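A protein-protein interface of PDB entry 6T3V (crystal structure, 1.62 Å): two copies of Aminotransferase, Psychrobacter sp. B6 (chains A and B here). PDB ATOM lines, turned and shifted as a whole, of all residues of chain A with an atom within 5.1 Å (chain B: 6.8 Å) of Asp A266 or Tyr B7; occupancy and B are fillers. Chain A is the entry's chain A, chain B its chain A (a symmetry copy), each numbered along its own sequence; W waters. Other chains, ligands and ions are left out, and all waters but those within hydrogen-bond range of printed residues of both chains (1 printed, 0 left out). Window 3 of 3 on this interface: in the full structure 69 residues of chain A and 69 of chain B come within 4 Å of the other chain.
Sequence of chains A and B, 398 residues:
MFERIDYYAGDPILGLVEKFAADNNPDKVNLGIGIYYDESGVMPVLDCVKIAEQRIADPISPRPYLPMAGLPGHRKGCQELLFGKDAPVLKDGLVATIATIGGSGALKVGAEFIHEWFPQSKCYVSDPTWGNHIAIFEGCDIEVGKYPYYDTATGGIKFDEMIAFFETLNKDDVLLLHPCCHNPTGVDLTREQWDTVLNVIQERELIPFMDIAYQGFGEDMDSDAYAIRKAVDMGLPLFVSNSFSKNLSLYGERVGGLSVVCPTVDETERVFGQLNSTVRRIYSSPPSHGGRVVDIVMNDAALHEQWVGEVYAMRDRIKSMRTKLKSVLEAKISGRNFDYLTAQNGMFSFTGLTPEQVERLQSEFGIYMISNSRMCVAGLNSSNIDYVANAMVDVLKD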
ATOM      1  N   THR A 264     -12.939  24.068  11.828  1.00  0.00           N
ATOM      2  CA  THR A 264     -12.332  22.917  12.535  1.00  0.00           C
ATOM      3  C   THR A 264     -12.217  23.199  14.044  1.00  0.00           C
ATOM      4  O   THR A 264     -12.219  24.353  14.474  1.00  0.00           O
ATOM      5  CB  THR A 264     -10.905  22.595  12.028  1.00  0.00           C
ATOM      6  OG1 THR A 264      -9.992  23.665  12.344  1.00  0.00           O
ATOM      7  CG2 THR A 264     -10.904  22.376  10.544  1.00  0.00           C
ATOM      8  N   VAL A 265     -12.085  22.135  14.834  1.00  0.00           N
ATOM      9  CA  VAL A 265     -11.917  22.233  16.280  1.00  0.00           C
ATOM     10  C   VAL A 265     -10.607  22.955  16.604  1.00  0.00           C
ATOM     11  O   VAL A 265     -10.557  23.746  17.537  1.00  0.00           O
ATOM     12  CB  VAL A 265     -11.981  20.819  16.931  1.00  0.00           C
ATOM     13  CG1 VAL A 265     -11.517  20.840  18.385  1.00  0.00           C
ATOM     14  CG2 VAL A 265     -13.407  20.353  16.900  1.00  0.00           C
ATOM     15  N   ASP A 266      -9.540  22.709  15.845  1.00  0.00           N
ATOM     16  CA  ASP A 266      -8.269  23.367  16.146  1.00  0.00           C
ATOM     17  C   ASP A 266      -8.401  24.884  15.912  1.00  0.00           C
ATOM     18  O   ASP A 266      -7.874  25.693  16.693  1.00  0.00           O
ATOM     19  CB  ASP A 266      -7.133  22.796  15.271  1.00  0.00           C
ATOM     20  CG  ASP A 266      -5.776  23.446  15.602  1.00  0.00           C
ATOM     21  OD1 ASP A 266      -5.295  23.265  16.752  1.00  0.00           O
ATOM     22  OD2 ASP A 266      -5.195  24.152  14.736  1.00  0.00           O
ATOM     23  N   GLU A 267      -9.120  25.273  14.863  1.00  0.00           N
ATOM     24  CA  GLU A 267      -9.324  26.720  14.621  1.00  0.00           C
ATOM     25  C   GLU A 267     -10.201  27.315  15.703  1.00  0.00           C
ATOM     26  O   GLU A 267      -9.967  28.456  16.119  1.00  0.00           O
ATOM     27  CB  GLU A 267      -9.907  26.986  13.221  1.00  0.00           C
ATOM     28  CG  GLU A 267      -8.860  26.778  12.104  1.00  0.00           C
ATOM     29  CD  GLU A 267      -9.523  26.714  10.749  1.00  0.00           C
ATOM     30  OE1 GLU A 267      -9.771  27.762  10.132  1.00  0.00           O
ATOM     31  OE2 GLU A 267      -9.868  25.602  10.316  1.00  0.00           O
ATOM     32  N   THR A 268     -11.206  26.572  16.172  1.00  0.00           N
ATOM     33  CA  THR A 268     -12.040  27.028  17.306  1.00  0.00           C
ATOM     34  C   THR A 268     -11.154  27.288  18.537  1.00  0.00           C
ATOM     35  O   THR A 268     -11.333  28.316  19.222  1.00  0.00           O
ATOM     36  CB  THR A 268     -13.139  26.007  17.644  1.00  0.00           C
ATOM     37  OG1 THR A 268     -13.873  25.732  16.462  1.00  0.00           O
ATOM     38  CG2 THR A 268     -14.128  26.570  18.673  1.00  0.00           C
ATOM     39  N   GLU A 269     -10.194  26.397  18.811  1.00  0.00           N
ATOM     40  CA  GLU A 269      -9.294  26.581  19.956  1.00  0.00           C
ATOM     41  C   GLU A 269      -8.411  27.835  19.782  1.00  0.00           C
ATOM     42  O   GLU A 269      -8.201  28.593  20.748  1.00  0.00           O
ATOM     43  CB  GLU A 269      -8.410  25.333  20.140  1.00  0.00           C
ATOM     44  CG  GLU A 269      -7.459  25.458  21.337  1.00  0.00           C
ATOM     45  CD  GLU A 269      -6.582  24.222  21.565  1.00  0.00           C
ATOM     46  OE1 GLU A 269      -6.894  23.134  21.032  1.00  0.00           O
ATOM     47  OE2 GLU A 269      -5.584  24.343  22.311  1.00  0.00           O
ATOM     48  N   ARG A 270      -7.881  28.032  18.570  1.00  0.00           N
ATOM     49  CA  ARG A 270      -7.051  29.217  18.289  1.00  0.00           C
ATOM     50  C   ARG A 270      -7.876  30.493  18.506  1.00  0.00           C
ATOM     51  O   ARG A 270      -7.452  31.415  19.217  1.00  0.00           O
ATOM     52  CB  ARG A 270      -6.550  29.144  16.867  1.00  0.00           C
ATOM     53  CG  ARG A 270      -5.525  28.028  16.675  1.00  0.00           C
ATOM     54  CD  ARG A 270      -5.245  27.897  15.203  1.00  0.00           C
ATOM     55  NE  ARG A 270      -4.250  26.825  14.948  1.00  0.00           N
ATOM     56  CZ  ARG A 270      -2.929  27.001  14.971  1.00  0.00           C
ATOM     57  NH1 ARG A 270      -2.390  28.211  15.224  1.00  0.00           N
ATOM     58  NH2 ARG A 270      -2.138  25.969  14.704  1.00  0.00           N
ATOM     59  N   GLN A 274      -7.616  33.415  21.502  1.00  0.00           N
ATOM     60  CA  GLN A 274      -7.360  34.823  21.191  1.00  0.00           C
ATOM     61  C   GLN A 274      -8.492  35.725  21.661  1.00  0.00           C
ATOM     62  O   GLN A 274      -8.236  36.891  22.030  1.00  0.00           O
ATOM     63  CB  GLN A 274      -7.042  35.035  19.693  1.00  0.00           C
ATOM     64  CG  GLN A 274      -5.654  34.474  19.336  1.00  0.00           C
ATOM     65  CD  GLN A 274      -4.511  35.042  20.179  1.00  0.00           C
ATOM     66  OE1 GLN A 274      -4.541  36.220  20.587  1.00  0.00           O
ATOM     67  NE2 GLN A 274      -3.486  34.225  20.415  1.00  0.00           N
ATOM     68  N   PHE B   2      -8.898  30.301   9.918  1.00  0.00           N
ATOM     69  CA  PHE B   2      -8.244  30.861  11.079  1.00  0.00           C
ATOM     70  C   PHE B   2      -6.920  30.173  11.409  1.00  0.00           C
ATOM     71  O   PHE B   2      -6.435  30.254  12.549  1.00  0.00           O
ATOM     72  CB  PHE B   2      -9.208  30.837  12.298  1.00  0.00           C
ATOM     73  CG  PHE B   2     -10.473  31.637  12.094  1.00  0.00           C
ATOM     74  CD1 PHE B   2     -10.435  33.045  11.982  1.00  0.00           C
ATOM     75  CD2 PHE B   2     -11.717  31.005  12.070  1.00  0.00           C
ATOM     76  CE1 PHE B   2     -11.618  33.779  11.810  1.00  0.00           C
ATOM     77  CE2 PHE B   2     -12.901  31.739  11.900  1.00  0.00           C
ATOM     78  CZ  PHE B   2     -12.853  33.140  11.784  1.00  0.00           C
ATOM     79  N   GLU B   3      -6.312  29.519  10.400  1.00  0.00           N
ATOM     80  CA  GLU B   3      -5.024  28.858  10.650  1.00  0.00           C
ATOM     81  C   GLU B   3      -3.931  29.875  11.022  1.00  0.00           C
ATOM     82  O   GLU B   3      -3.037  29.522  11.763  1.00  0.00           O
ATOM     83  CB  GLU B   3      -4.599  27.918   9.498  1.00  0.00           C
ATOM     84  CG  GLU B   3      -5.549  26.739   9.309  1.00  0.00           C
ATOM     85  CD  GLU B   3      -5.127  25.792   8.186  1.00  0.00           C
ATOM     86  OE1 GLU B   3      -3.914  25.505   8.040  1.00  0.00           O
ATOM     87  OE2 GLU B   3      -6.023  25.316   7.453  1.00  0.00           O
ATOM     88  N   ILE B   5      -4.164  32.184  13.107  1.00  0.00           N
ATOM     89  CA  ILE B   5      -4.380  32.693  14.475  1.00  0.00           C
ATOM     90  C   ILE B   5      -3.557  31.844  15.454  1.00  0.00           C
ATOM     91  O   ILE B   5      -3.781  30.634  15.572  1.00  0.00           O
ATOM     92  CB  ILE B   5      -5.878  32.648  14.878  1.00  0.00           C
ATOM     93  CG1 ILE B   5      -6.840  33.280  13.820  1.00  0.00           C
ATOM     94  CG2 ILE B   5      -6.107  33.247  16.271  1.00  0.00           C
ATOM     95  CD1 ILE B   5      -6.689  34.764  13.554  1.00  0.00           C
ATOM     96  N   ASP B   6      -2.630  32.487  16.173  1.00  0.00           N
ATOM     97  CA  ASP B   6      -1.786  31.827  17.175  1.00  0.00           C
ATOM     98  C   ASP B   6      -2.642  31.255  18.289  1.00  0.00           C
ATOM     99  O   ASP B   6      -3.675  31.847  18.684  1.00  0.00           O
ATOM    100  CB  ASP B   6      -0.797  32.804  17.847  1.00  0.00           C
ATOM    101  CG  ASP B   6       0.220  33.417  16.882  1.00  0.00           C
ATOM    102  OD1 ASP B   6       0.336  32.998  15.694  1.00  0.00           O
ATOM    103  OD2 ASP B   6       0.934  34.349  17.347  1.00  0.00           O
ATOM    104  N   TYR B   7      -2.200  30.130  18.835  1.00  0.00           N
ATOM    105  CA  TYR B   7      -2.722  29.714  20.117  1.00  0.00           C
ATOM    106  C   TYR B   7      -2.385  30.760  21.139  1.00  0.00           C
ATOM    107  O   TYR B   7      -1.321  31.403  21.080  1.00  0.00           O
ATOM    108  CB  TYR B   7      -2.093  28.382  20.592  1.00  0.00           C
ATOM    109  CG  TYR B   7      -2.371  27.235  19.693  1.00  0.00           C
ATOM    110  CD1 TYR B   7      -3.663  26.713  19.564  1.00  0.00           C
ATOM    111  CD2 TYR B   7      -1.331  26.642  18.967  1.00  0.00           C
ATOM    112  CE1 TYR B   7      -3.923  25.630  18.703  1.00  0.00           C
ATOM    113  CE2 TYR B   7      -1.569  25.572  18.117  1.00  0.00           C
ATOM    114  CZ  TYR B   7      -2.854  25.068  17.984  1.00  0.00           C
ATOM    115  OH  TYR B   7      -3.056  23.983  17.171  1.00  0.00           O
ATOM    116  N   TYR B   8      -3.292  30.936  22.083  1.00  0.00           N
ATOM    117  CA  TYR B   8      -2.968  31.763  23.215  1.00  0.00           C
ATOM    118  C   TYR B   8      -2.375  30.848  24.237  1.00  0.00           C
ATOM    119  O   TYR B   8      -2.983  29.835  24.582  1.00  0.00           O
ATOM    120  CB  TYR B   8      -4.219  32.460  23.720  1.00  0.00           C
ATOM    121  CG  TYR B   8      -4.088  33.383  24.947  1.00  0.00           C
ATOM    122  CD1 TYR B   8      -3.037  34.306  25.083  1.00  0.00           C
ATOM    123  CD2 TYR B   8      -5.118  33.417  25.897  1.00  0.00           C
ATOM    124  CE1 TYR B   8      -2.972  35.180  26.187  1.00  0.00           C
ATOM    125  CE2 TYR B   8      -5.047  34.272  26.996  1.00  0.00           C
ATOM    126  CZ  TYR B   8      -4.015  35.179  27.111  1.00  0.00           C
ATOM    127  OH  TYR B   8      -4.046  36.056  28.209  1.00  0.00           O
ATOM    128  N   ALA B   9      -1.165  31.197  24.689  1.00  0.00           N
ATOM    129  CA  ALA B   9      -0.444  30.484  25.757  1.00  0.00           C
ATOM    130  C   ALA B   9      -1.171  30.528  27.123  1.00  0.00           C
ATOM    131  O   ALA B   9      -0.955  29.645  27.955  1.00  0.00           O
ATOM    132  CB  ALA B   9       0.982  31.034  25.885  1.00  0.00           C
ATOM    133  N   GLY B  10      -2.040  31.529  27.318  1.00  0.00           N
ATOM    134  CA  GLY B  10      -2.821  31.761  28.559  1.00  0.00           C
ATOM    135  C   GLY B  10      -2.051  32.822  29.394  1.00  0.00           C
ATOM    136  O   GLY B  10      -0.910  33.061  29.131  1.00  0.00           O
HETATM  137  O   HOH W   1      -5.633  28.949  22.006  1.00  0.00           O
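NH2 of Arg A270 is in hydrogen-bond range of OH of Tyr B7. NE2 of Gln A274 sits at hydrogen-bond distance from O of Asp B6 (2.9 Å). The guanidinium group (NH1) of Arg A270 lies within hydrogen-bond range of the backbone carbonyl oxygen (O) of Ile B5 (2.8 Å). The side-chain carboxylate (OE1) of Glu A267 lies within hydrogen-bond range of the backbone NH (N) of Phe B2. The side-chain hydroxyl (OH) of Tyr B7 sits close to the side-chain carboxylate (OD2) of Asp A266 (3.2 Å).
The side-chain carboxylate of Glu A267 sits at hydrogen-bond distance from the side-chain hydroxyl of Thr A264. The side-chain carboxylate of Asp A266 lies within salt-bridge range of the guanidinium group of Arg A270, 2.8 Å away.
Among the printed residues, merely in contact across the chains: Gln A274 with Ile B5 (3.3 Å), Gln A274 with Tyr B7 (3.6 Å), Gln A274 with Tyr B8 (3.7 Å), Arg A270 with Phe B2 (3.7 Å), Arg A270 with Glu B3 (3.8 Å), Arg A270 with Asp B6 (3.8 Å) and Glu A267 with Glu B3 (3.9 Å).
Printed residues of chain B within 4 Å of Arg A270: Phe B2 (3.7 Å), Glu B3 (3.8 Å), Ile B5 (2.8 Å), Asp B6 (3.8 Å) and Tyr B7 (3.3 Å). Of the printed residues of chain A, Phe B2 touches Glu A267 and Arg A270. Printed residues of chain A within 4 Å of Ile B5: Arg A270 and Gln A274. Tyr B7 touches just these residues of chain A: Asp A266 (2.4 Å), Arg A270 (3.3 Å) and Gln A274 (3.6 Å). The nearest residue of chain B that does not touch Asp A266 is Glu B3 (6.0 Å). The nearest printed residue of chain B that does not touch Gln A274 is Ala B9 (5.7 Å).
No position is printed for both chains. Of the 12 pairs that touch across the chains among the printed residues, none has its exchanged pair printed and touching as well.
Water W1 lies within hydrogen-bond range of O of Glu A269 and N of Tyr B8.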
